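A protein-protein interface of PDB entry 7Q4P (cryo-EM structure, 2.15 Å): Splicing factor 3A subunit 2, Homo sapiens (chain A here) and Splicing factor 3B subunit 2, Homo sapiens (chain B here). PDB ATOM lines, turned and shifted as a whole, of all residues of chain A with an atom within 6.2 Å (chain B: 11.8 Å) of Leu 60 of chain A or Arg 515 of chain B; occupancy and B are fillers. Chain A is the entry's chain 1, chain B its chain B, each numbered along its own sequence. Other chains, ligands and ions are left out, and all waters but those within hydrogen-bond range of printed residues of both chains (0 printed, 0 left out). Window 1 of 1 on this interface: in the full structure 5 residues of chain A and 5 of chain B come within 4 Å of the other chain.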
ATOM      1  N   MET A  47     -14.525 -37.867  20.204  1.00  0.00           N
ATOM      2  CA  MET A  47     -15.750 -37.425  20.846  1.00  0.00           C
ATOM      3  C   MET A  47     -16.933 -38.040  20.112  1.00  0.00           C
ATOM      4  O   MET A  47     -16.891 -38.216  18.895  1.00  0.00           O
ATOM      5  CB  MET A  47     -15.879 -35.898  20.860  1.00  0.00           C
ATOM      6  CG  MET A  47     -15.655 -35.237  19.513  1.00  0.00           C
ATOM      7  SD  MET A  47     -16.394 -33.584  19.453  1.00  0.00           S
ATOM      8  CE  MET A  47     -18.106 -33.988  19.106  1.00  0.00           C
ATOM      9  N   GLU A  55     -16.474 -37.955  16.042  1.00  0.00           N
ATOM     10  CA  GLU A  55     -15.758 -36.847  15.431  1.00  0.00           C
ATOM     11  C   GLU A  55     -14.324 -36.831  15.949  1.00  0.00           C
ATOM     12  O   GLU A  55     -14.062 -37.233  17.081  1.00  0.00           O
ATOM     13  CB  GLU A  55     -16.432 -35.533  15.827  1.00  0.00           C
ATOM     14  CG  GLU A  55     -17.875 -35.426  15.368  1.00  0.00           C
ATOM     15  CD  GLU A  55     -18.421 -34.009  15.334  1.00  0.00           C
ATOM     16  OE1 GLU A  55     -17.780 -33.154  14.698  1.00  0.00           O
ATOM     17  OE2 GLU A  55     -19.477 -33.761  15.947  1.00  0.00           O
ATOM     18  N   CYS A  56     -13.390 -36.378  15.107  1.00  0.00           N
ATOM     19  CA  CYS A  56     -12.074 -35.956  15.553  1.00  0.00           C
ATOM     20  C   CYS A  56     -12.096 -34.455  15.848  1.00  0.00           C
ATOM     21  O   CYS A  56     -12.587 -33.665  15.050  1.00  0.00           O
ATOM     22  CB  CYS A  56     -11.048 -36.300  14.484  1.00  0.00           C
ATOM     23  SG  CYS A  56      -9.339 -36.001  15.006  1.00  0.00           S
ATOM     24  N   LYS A  57     -11.589 -34.074  17.023  1.00  0.00           N
ATOM     25  CA  LYS A  57     -11.639 -32.687  17.456  1.00  0.00           C
ATOM     26  C   LYS A  57     -10.476 -31.921  16.844  1.00  0.00           C
ATOM     27  O   LYS A  57     -10.535 -30.700  16.708  1.00  0.00           O
ATOM     28  CB  LYS A  57     -11.474 -32.596  18.971  1.00  0.00           C
ATOM     29  CG  LYS A  57     -12.692 -32.972  19.793  1.00  0.00           C
ATOM     30  CD  LYS A  57     -12.697 -32.322  21.162  1.00  0.00           C
ATOM     31  CE  LYS A  57     -13.634 -32.991  22.145  1.00  0.00           C
ATOM     32  NZ  LYS A  57     -13.174 -34.358  22.482  1.00  0.00           N
ATOM     33  N   LEU A  58      -9.413 -32.659  16.507  1.00  0.00           N
ATOM     34  CA  LEU A  58      -8.181 -32.068  16.026  1.00  0.00           C
ATOM     35  C   LEU A  58      -8.305 -31.692  14.550  1.00  0.00           C
ATOM     36  O   LEU A  58      -7.805 -30.646  14.134  1.00  0.00           O
ATOM     37  CB  LEU A  58      -7.081 -33.106  16.249  1.00  0.00           C
ATOM     38  CG  LEU A  58      -5.651 -32.675  15.962  1.00  0.00           C
ATOM     39  CD1 LEU A  58      -5.148 -31.686  17.003  1.00  0.00           C
ATOM     40  CD2 LEU A  58      -4.753 -33.899  15.918  1.00  0.00           C
ATOM     41  N   CYS A  59      -8.951 -32.573  13.772  1.00  0.00           N
ATOM     42  CA  CYS A  59      -8.983 -32.481  12.318  1.00  0.00           C
ATOM     43  C   CYS A  59     -10.343 -31.981  11.832  1.00  0.00           C
ATOM     44  O   CYS A  59     -10.431 -31.445  10.724  1.00  0.00           O
ATOM     45  CB  CYS A  59      -8.677 -33.831  11.678  1.00  0.00           C
ATOM     46  SG  CYS A  59      -7.029 -34.483  12.060  1.00  0.00           S
ATOM     47  N   LEU A  60     -11.370 -32.165  12.682  1.00  0.00           N
ATOM     48  CA  LEU A  60     -12.765 -31.845  12.405  1.00  0.00           C
ATOM     49  C   LEU A  60     -13.241 -32.703  11.237  1.00  0.00           C
ATOM     50  O   LEU A  60     -13.531 -32.216  10.149  1.00  0.00           O
ATOM     51  CB  LEU A  60     -12.957 -30.344  12.155  1.00  0.00           C
ATOM     52  CG  LEU A  60     -12.542 -29.403  13.286  1.00  0.00           C
ATOM     53  CD1 LEU A  60     -12.522 -27.965  12.800  1.00  0.00           C
ATOM     54  CD2 LEU A  60     -13.445 -29.544  14.506  1.00  0.00           C
ATOM     55  N   THR A  61     -13.230 -34.014  11.478  1.00  0.00           N
ATOM     56  CA  THR A  61     -13.586 -35.013  10.492  1.00  0.00           C
ATOM     57  C   THR A  61     -14.629 -35.916  11.125  1.00  0.00           C
ATOM     58  O   THR A  61     -14.526 -36.264  12.295  1.00  0.00           O
ATOM     59  CB  THR A  61     -12.365 -35.823  10.032  1.00  0.00           C
ATOM     60  OG1 THR A  61     -11.573 -36.214  11.154  1.00  0.00           O
ATOM     61  CG2 THR A  61     -11.500 -35.074   9.041  1.00  0.00           C
ATOM     62  N   LEU A  62     -15.594 -36.354  10.325  1.00  0.00           N
ATOM     63  CA  LEU A  62     -16.690 -37.135  10.873  1.00  0.00           C
ATOM     64  C   LEU A  62     -16.444 -38.604  10.574  1.00  0.00           C
ATOM     65  O   LEU A  62     -15.936 -38.942   9.498  1.00  0.00           O
ATOM     66  CB  LEU A  62     -18.005 -36.695  10.233  1.00  0.00           C
ATOM     67  CG  LEU A  62     -18.362 -35.213  10.321  1.00  0.00           C
ATOM     68  CD1 LEU A  62     -19.652 -34.948   9.557  1.00  0.00           C
ATOM     69  CD2 LEU A  62     -18.517 -34.749  11.764  1.00  0.00           C
ATOM     70  N   HIS A  72      -8.430 -43.205  10.295  1.00  0.00           N
ATOM     71  CA  HIS A  72      -8.162 -41.787  10.117  1.00  0.00           C
ATOM     72  C   HIS A  72      -6.882 -41.396  10.853  1.00  0.00           C
ATOM     73  O   HIS A  72      -6.117 -40.578  10.349  1.00  0.00           O
ATOM     74  CB  HIS A  72      -9.389 -40.962  10.537  1.00  0.00           C
ATOM     75  CG  HIS A  72      -9.075 -39.552  10.929  1.00  0.00           C
ATOM     76  ND1 HIS A  72      -8.819 -38.571   9.994  1.00  0.00           N
ATOM     77  CD2 HIS A  72      -8.958 -38.951  12.136  1.00  0.00           C
ATOM     78  CE1 HIS A  72      -8.546 -37.433  10.598  1.00  0.00           C
ATOM     79  NE2 HIS A  72      -8.635 -37.635  11.909  1.00  0.00           N
ATOM     80  N   LYS A  77      -3.837 -36.723   7.409  1.00  0.00           N
ATOM     81  CA  LYS A  77      -4.463 -35.534   7.966  1.00  0.00           C
ATOM     82  C   LYS A  77      -4.285 -35.489   9.484  1.00  0.00           C
ATOM     83  O   LYS A  77      -4.151 -34.409  10.056  1.00  0.00           O
ATOM     84  CB  LYS A  77      -5.941 -35.502   7.559  1.00  0.00           C
ATOM     85  CG  LYS A  77      -6.671 -34.180   7.781  1.00  0.00           C
ATOM     86  CD  LYS A  77      -8.033 -34.110   7.117  1.00  0.00           C
ATOM     87  CE  LYS A  77      -8.745 -32.798   7.369  1.00  0.00           C
ATOM     88  NZ  LYS A  77     -10.073 -32.757   6.710  1.00  0.00           N
ATOM     89  N   LYS B 507     -17.392 -21.908   0.035  1.00  0.00           N
ATOM     90  CA  LYS B 507     -17.026 -23.171  -0.599  1.00  0.00           C
ATOM     91  C   LYS B 507     -17.653 -24.346   0.149  1.00  0.00           C
ATOM     92  O   LYS B 507     -18.141 -25.301  -0.456  1.00  0.00           O
ATOM     93  CB  LYS B 507     -15.505 -23.352  -0.644  1.00  0.00           C
ATOM     94  CG  LYS B 507     -14.743 -22.314  -1.454  1.00  0.00           C
ATOM     95  CD  LYS B 507     -14.917 -22.452  -2.950  1.00  0.00           C
ATOM     96  CE  LYS B 507     -14.274 -21.321  -3.722  1.00  0.00           C
ATOM     97  NZ  LYS B 507     -14.534 -21.438  -5.176  1.00  0.00           N
ATOM     98  N   ARG B 508     -17.631 -24.261   1.483  1.00  0.00           N
ATOM     99  CA  ARG B 508     -18.174 -25.313   2.343  1.00  0.00           C
ATOM    100  C   ARG B 508     -19.707 -25.309   2.238  1.00  0.00           C
ATOM    101  O   ARG B 508     -20.280 -24.244   2.039  1.00  0.00           O
ATOM    102  CB  ARG B 508     -17.658 -25.067   3.768  1.00  0.00           C
ATOM    103  CG  ARG B 508     -18.062 -26.095   4.813  1.00  0.00           C
ATOM    104  CD  ARG B 508     -17.069 -27.180   5.189  1.00  0.00           C
ATOM    105  NE  ARG B 508     -16.022 -26.771   6.123  1.00  0.00           N
ATOM    106  CZ  ARG B 508     -15.328 -27.583   6.923  1.00  0.00           C
ATOM    107  NH1 ARG B 508     -15.597 -28.878   6.973  1.00  0.00           N
ATOM    108  NH2 ARG B 508     -14.361 -27.089   7.674  1.00  0.00           N
ATOM    109  N   LYS B 509     -20.377 -26.479   2.354  1.00  0.00           N
ATOM    110  CA  LYS B 509     -21.838 -26.534   2.316  1.00  0.00           C
ATOM    111  C   LYS B 509     -22.438 -25.864   3.552  1.00  0.00           C
ATOM    112  O   LYS B 509     -21.691 -25.389   4.398  1.00  0.00           O
ATOM    113  CB  LYS B 509     -22.352 -27.968   2.163  1.00  0.00           C
ATOM    114  CG  LYS B 509     -21.747 -28.749   1.016  1.00  0.00           C
ATOM    115  CD  LYS B 509     -22.363 -28.429  -0.329  1.00  0.00           C
ATOM    116  CE  LYS B 509     -21.985 -29.435  -1.393  1.00  0.00           C
ATOM    117  NZ  LYS B 509     -22.609 -29.121  -2.702  1.00  0.00           N
ATOM    118  N   TYR B 510     -23.777 -25.792   3.631  1.00  0.00           N
ATOM    119  CA  TYR B 510     -24.453 -24.827   4.487  1.00  0.00           C
ATOM    120  C   TYR B 510     -24.138 -25.017   5.968  1.00  0.00           C
ATOM    121  O   TYR B 510     -23.852 -24.077   6.673  1.00  0.00           O
ATOM    122  CB  TYR B 510     -25.951 -24.694   4.190  1.00  0.00           C
ATOM    123  CG  TYR B 510     -26.754 -24.036   5.273  1.00  0.00           C
ATOM    124  CD1 TYR B 510     -26.327 -22.870   5.888  1.00  0.00           C
ATOM    125  CD2 TYR B 510     -27.927 -24.625   5.687  1.00  0.00           C
ATOM    126  CE1 TYR B 510     -27.081 -22.288   6.896  1.00  0.00           C
ATOM    127  CE2 TYR B 510     -28.703 -24.043   6.677  1.00  0.00           C
ATOM    128  CZ  TYR B 510     -28.277 -22.872   7.288  1.00  0.00           C
ATOM    129  OH  TYR B 510     -29.020 -22.324   8.298  1.00  0.00           O
ATOM    130  N   LEU B 511     -24.196 -26.209   6.513  1.00  0.00           N
ATOM    131  CA  LEU B 511     -23.850 -26.196   7.933  1.00  0.00           C
ATOM    132  C   LEU B 511     -22.688 -27.110   8.320  1.00  0.00           C
ATOM    133  O   LEU B 511     -22.633 -27.617   9.439  1.00  0.00           O
ATOM    134  CB  LEU B 511     -25.140 -26.615   8.641  1.00  0.00           C
ATOM    135  CG  LEU B 511     -26.137 -25.490   8.897  1.00  0.00           C
ATOM    136  CD1 LEU B 511     -27.473 -25.947   9.480  1.00  0.00           C
ATOM    137  CD2 LEU B 511     -25.452 -24.458   9.742  1.00  0.00           C
ATOM    138  N   GLN B 512     -21.938 -27.555   7.314  1.00  0.00           N
ATOM    139  CA  GLN B 512     -21.023 -28.678   7.314  1.00  0.00           C
ATOM    140  C   GLN B 512     -19.891 -28.301   8.237  1.00  0.00           C
ATOM    141  O   GLN B 512     -19.351 -29.150   8.914  1.00  0.00           O
ATOM    142  CB  GLN B 512     -20.810 -29.111   5.865  1.00  0.00           C
ATOM    143  CG  GLN B 512     -22.070 -29.765   5.307  1.00  0.00           C
ATOM    144  CD  GLN B 512     -22.664 -30.907   6.106  1.00  0.00           C
ATOM    145  OE1 GLN B 512     -23.849 -30.886   6.445  1.00  0.00           O
ATOM    146  NE2 GLN B 512     -21.846 -31.900   6.428  1.00  0.00           N
ATOM    147  N   GLY B 513     -19.664 -26.999   8.341  1.00  0.00           N
ATOM    148  CA  GLY B 513     -18.624 -26.482   9.199  1.00  0.00           C
ATOM    149  C   GLY B 513     -18.940 -26.590  10.697  1.00  0.00           C
ATOM    150  O   GLY B 513     -18.065 -26.284  11.506  1.00  0.00           O
ATOM    151  N   LYS B 514     -20.141 -27.066  11.077  1.00  0.00           N
ATOM    152  CA  LYS B 514     -20.462 -27.258  12.489  1.00  0.00           C
ATOM    153  C   LYS B 514     -20.051 -28.675  12.875  1.00  0.00           C
ATOM    154  O   LYS B 514     -20.783 -29.625  12.601  1.00  0.00           O
ATOM    155  CB  LYS B 514     -21.961 -27.107  12.788  1.00  0.00           C
ATOM    156  CG  LYS B 514     -22.625 -25.773  12.461  1.00  0.00           C
ATOM    157  CD  LYS B 514     -24.070 -25.725  12.888  1.00  0.00           C
ATOM    158  CE  LYS B 514     -24.255 -25.673  14.391  1.00  0.00           C
ATOM    159  NZ  LYS B 514     -25.684 -25.553  14.762  1.00  0.00           N
ATOM    160  N   ARG B 515     -18.881 -28.787  13.508  1.00  0.00           N
ATOM    161  CA  ARG B 515     -18.256 -30.051  13.866  1.00  0.00           C
ATOM    162  C   ARG B 515     -17.246 -29.790  14.982  1.00  0.00           C
ATOM    163  O   ARG B 515     -16.787 -28.660  15.125  1.00  0.00           O
ATOM    164  CB  ARG B 515     -17.647 -30.740  12.635  1.00  0.00           C
ATOM    165  CG  ARG B 515     -16.873 -29.843  11.676  1.00  0.00           C
ATOM    166  CD  ARG B 515     -16.465 -30.753  10.520  1.00  0.00           C
ATOM    167  NE  ARG B 515     -17.588 -31.258   9.727  1.00  0.00           N
ATOM    168  CZ  ARG B 515     -17.507 -32.053   8.662  1.00  0.00           C
ATOM    169  NH1 ARG B 515     -16.330 -32.467   8.221  1.00  0.00           N
ATOM    170  NH2 ARG B 515     -18.607 -32.397   8.013  1.00  0.00           N
ATOM    171  N   GLY B 516     -16.931 -30.835  15.765  1.00  0.00           N
ATOM    172  CA  GLY B 516     -16.023 -30.756  16.902  1.00  0.00           C
ATOM    173  C   GLY B 516     -16.620 -30.021  18.101  1.00  0.00           C
ATOM    174  O   GLY B 516     -15.885 -29.611  19.002  1.00  0.00           O
ATOM    175  N   ILE B 517     -17.954 -29.883  18.118  1.00  0.00           N
ATOM    176  CA  ILE B 517     -18.676 -29.238  19.205  1.00  0.00           C
ATOM    177  C   ILE B 517     -19.479 -30.302  19.950  1.00  0.00           C
ATOM    178  O   ILE B 517     -20.275 -31.008  19.338  1.00  0.00           O
ATOM    179  CB  ILE B 517     -19.604 -28.135  18.645  1.00  0.00           C
ATOM    180  CG1 ILE B 517     -18.923 -27.268  17.578  1.00  0.00           C
ATOM    181  CG2 ILE B 517     -20.223 -27.313  19.772  1.00  0.00           C
ATOM    182  CD1 ILE B 517     -19.876 -26.398  16.779  1.00  0.00           C
ATOM    183  N   GLU B 518     -19.285 -30.386  21.273  1.00  0.00           N
ATOM    184  CA  GLU B 518     -20.077 -31.262  22.121  1.00  0.00           C
ATOM    185  C   GLU B 518     -21.279 -30.477  22.643  1.00  0.00           C
ATOM    186  O   GLU B 518     -21.335 -30.125  23.823  1.00  0.00           O
ATOM    187  CB  GLU B 518     -19.216 -31.858  23.241  1.00  0.00           C
ATOM    188  CG  GLU B 518     -18.340 -33.015  22.788  1.00  0.00           C
ATOM    189  CD  GLU B 518     -17.605 -33.750  23.896  1.00  0.00           C
ATOM    190  OE1 GLU B 518     -16.850 -33.095  24.645  1.00  0.00           O
ATOM    191  OE2 GLU B 518     -17.789 -34.979  24.010  1.00  0.00           O
ATOM    192  N   LYS B 519     -22.236 -30.203  21.746  1.00  0.00           N
ATOM    193  CA  LYS B 519     -23.442 -29.468  22.096  1.00  0.00           C
ATOM    194  C   LYS B 519     -24.322 -30.327  23.004  1.00  0.00           C
ATOM    195  O   LYS B 519     -24.456 -31.533  22.773  1.00  0.00           O
ATOM    196  CB  LYS B 519     -24.156 -28.911  20.858  1.00  0.00           C
ATOM    197  CG  LYS B 519     -24.741 -29.935  19.893  1.00  0.00           C
ATOM    198  CD  LYS B 519     -25.922 -29.415  19.096  1.00  0.00           C
ATOM    199  CE  LYS B 519     -27.259 -29.925  19.598  1.00  0.00           C
ATOM    200  NZ  LYS B 519     -28.387 -29.383  18.802  1.00  0.00           N
ATOM    201  N   TYR B 591     -31.020 -17.361  10.159  1.00  0.00           N
ATOM    202  CA  TYR B 591     -30.005 -18.068  10.937  1.00  0.00           C
ATOM    203  C   TYR B 591     -28.775 -18.336  10.067  1.00  0.00           C
ATOM    204  O   TYR B 591     -28.952 -18.655   8.895  1.00  0.00           O
ATOM    205  CB  TYR B 591     -30.538 -19.393  11.495  1.00  0.00           C
ATOM    206  CG  TYR B 591     -29.508 -20.176  12.273  1.00  0.00           C
ATOM    207  CD1 TYR B 591     -29.190 -19.811  13.569  1.00  0.00           C
ATOM    208  CD2 TYR B 591     -28.807 -21.225  11.695  1.00  0.00           C
ATOM    209  CE1 TYR B 591     -28.228 -20.494  14.297  1.00  0.00           C
ATOM    210  CE2 TYR B 591     -27.835 -21.913  12.406  1.00  0.00           C
ATOM    211  CZ  TYR B 591     -27.552 -21.552  13.714  1.00  0.00           C
ATOM    212  OH  TYR B 591     -26.594 -22.215  14.425  1.00  0.00           O
ATOM    213  N   TYR B 592     -27.564 -18.201  10.634  1.00  0.00           N
ATOM    214  CA  TYR B 592     -26.299 -18.502   9.959  1.00  0.00           C
ATOM    215  C   TYR B 592     -25.499 -19.377  10.922  1.00  0.00           C
ATOM    216  O   TYR B 592     -25.872 -19.428  12.088  1.00  0.00           O
ATOM    217  CB  TYR B 592     -25.574 -17.234   9.477  1.00  0.00           C
ATOM    218  CG  TYR B 592     -25.411 -16.145  10.506  1.00  0.00           C
ATOM    219  CD1 TYR B 592     -24.239 -16.035  11.245  1.00  0.00           C
ATOM    220  CD2 TYR B 592     -26.407 -15.208  10.717  1.00  0.00           C
ATOM    221  CE1 TYR B 592     -24.069 -15.032  12.184  1.00  0.00           C
ATOM    222  CE2 TYR B 592     -26.255 -14.202  11.660  1.00  0.00           C
ATOM    223  CZ  TYR B 592     -25.084 -14.117  12.397  1.00  0.00           C
ATOM    224  OH  TYR B 592     -24.913 -13.138  13.333  1.00  0.00           O
ATOM    225  N   GLU B 593     -24.433 -20.045  10.457  1.00  0.00           N
ATOM    226  CA  GLU B 593     -23.669 -21.008  11.245  1.00  0.00           C
ATOM    227  C   GLU B 593     -23.200 -20.458  12.596  1.00  0.00           C
ATOM    228  O   GLU B 593     -23.320 -21.139  13.619  1.00  0.00           O
ATOM    229  CB  GLU B 593     -22.514 -21.558  10.410  1.00  0.00           C
ATOM    230  CG  GLU B 593     -21.577 -22.471  11.190  1.00  0.00           C
ATOM    231  CD  GLU B 593     -20.720 -23.415  10.361  1.00  0.00           C
ATOM    232  OE1 GLU B 593     -19.481 -23.367  10.530  1.00  0.00           O
ATOM    233  OE2 GLU B 593     -21.288 -24.186   9.538  1.00  0.00           O
ATOM    234  N   GLY B 594     -22.643 -19.239  12.585  1.00  0.00           N
ATOM    235  CA  GLY B 594     -22.045 -18.620  13.761  1.00  0.00           C
ATOM    236  C   GLY B 594     -23.002 -17.812  14.648  1.00  0.00           C
ATOM    237  O   GLY B 594     -22.563 -17.313  15.689  1.00  0.00           O
ATOM    238  N   GLU B 596     -25.741 -18.697  16.581  1.00  0.00           N
ATOM    239  CA  GLU B 596     -26.028 -19.316  17.865  1.00  0.00           C
ATOM    240  C   GLU B 596     -24.962 -18.961  18.907  1.00  0.00           C
ATOM    241  O   GLU B 596     -25.300 -18.613  20.035  1.00  0.00           O
ATOM    242  CB  GLU B 596     -26.171 -20.818  17.649  1.00  0.00           C
ATOM    243  CG  GLU B 596     -26.721 -21.542  18.859  1.00  0.00           C
ATOM    244  CD  GLU B 596     -26.875 -23.043  18.702  1.00  0.00           C
ATOM    245  OE1 GLU B 596     -26.739 -23.544  17.567  1.00  0.00           O
ATOM    246  OE2 GLU B 596     -27.139 -23.711  19.721  1.00  0.00           O
ATOM    247  N   PHE B 597     -23.683 -19.079  18.523  1.00  0.00           N
ATOM    248  CA  PHE B 597     -22.548 -18.883  19.411  1.00  0.00           C
ATOM    249  C   PHE B 597     -21.985 -17.469  19.207  1.00  0.00           C
ATOM    250  O   PHE B 597     -22.779 -16.505  19.228  1.00  0.00           O
ATOM    251  CB  PHE B 597     -21.490 -19.971  19.177  1.00  0.00           C
ATOM    252  CG  PHE B 597     -22.002 -21.274  18.605  1.00  0.00           C
ATOM    253  CD1 PHE B 597     -22.579 -22.240  19.422  1.00  0.00           C
ATOM    254  CD2 PHE B 597     -21.906 -21.537  17.242  1.00  0.00           C
ATOM    255  CE1 PHE B 597     -23.061 -23.429  18.890  1.00  0.00           C
ATOM    256  CE2 PHE B 597     -22.380 -22.730  16.711  1.00  0.00           C
ATOM    257  CZ  PHE B 597     -22.952 -23.676  17.537  1.00  0.00           C
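Among the printed residues, pairs that only touch across the chains: Leu 62 of chain A with Arg 515 of chain B (3.2 Å), Glu 55 of chain A with Arg 515 of chain B (3.2 Å), Met 47 of chain A with Ile 517 of chain B (3.7 Å), Leu 60 of chain A with Gly 516 of chain B (3.7 Å), Met 47 of chain A with Glu 518 of chain B (3.8 Å) and Met 47 of chain A with Gly 516 of chain B (3.8 Å).
Of the 11 printed residues of chain A, 4 touch a printed residue of chain B. Hydrophobic or aromatic side chains of chain A that line the printed part of chain B: Met 47, Leu 60 and Leu 62. Among the printed residues, 8 pairs touch across the chains. Among the printed residues, no Asp or Glu carboxylate lies within 4 Å of a Lys or Arg side-chain nitrogen of the other chain.
Leu 60 of chain A touches just these residues of chain B: Arg 515 (3.3 Å) and Gly 516 (3.7 Å). No residue of chain B comes within 4 Å of Cys 56 of chain A. No residue of chain B comes within 4 Å of Leu 58 of chain A. No residue of chain B comes within 4 Å of Cys 59 of chain A. No residue of chain B comes within 4 Å of Thr 61 of chain A. Printed residues of chain B within 4 Å of Leu 62 of chain A: Arg 515 (3.2 Å). Printed residues of chain A within 4 Å of Glu 518 of chain B: Met 47. Printed residues of chain B within 4 Å of Glu 55 of chain A: Arg 515 (3.2 Å) and Gly 516 (2.7 Å). Lys 514 of chain B touches none of the printed residues of chain A. The nearest residue of chain B that does not touch Leu 60 of chain A is Arg 508 of chain B (5.0 Å). The nearest printed residue of chain A that does not touch Ile 517 of chain B is Glu 55 of chain A (4.4 Å).
The backbone carbonyl oxygen (O) of Gln 512 of chain B lies within hydrogen-bond range of the guanidinium group (NE) of Arg 515 of chain B, at 2.9 Å. The backbone carbonyl oxygen (O) of Met 47 of chain A is in hydrogen-bond range of the backbone NH (N) of Glu 55 of chain A (2.9 Å).
The side-chain carboxylate (OE1) of Glu 55 of chain A is in hydrogen-bond range of the backbone NH (N) of Gly 516 of chain B (2.7 Å). The guanidinium group (NH1) of Arg 515 of chain B sits close to the backbone carbonyl oxygen (O) of Leu 60 of chain A, 3.4 Å away.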
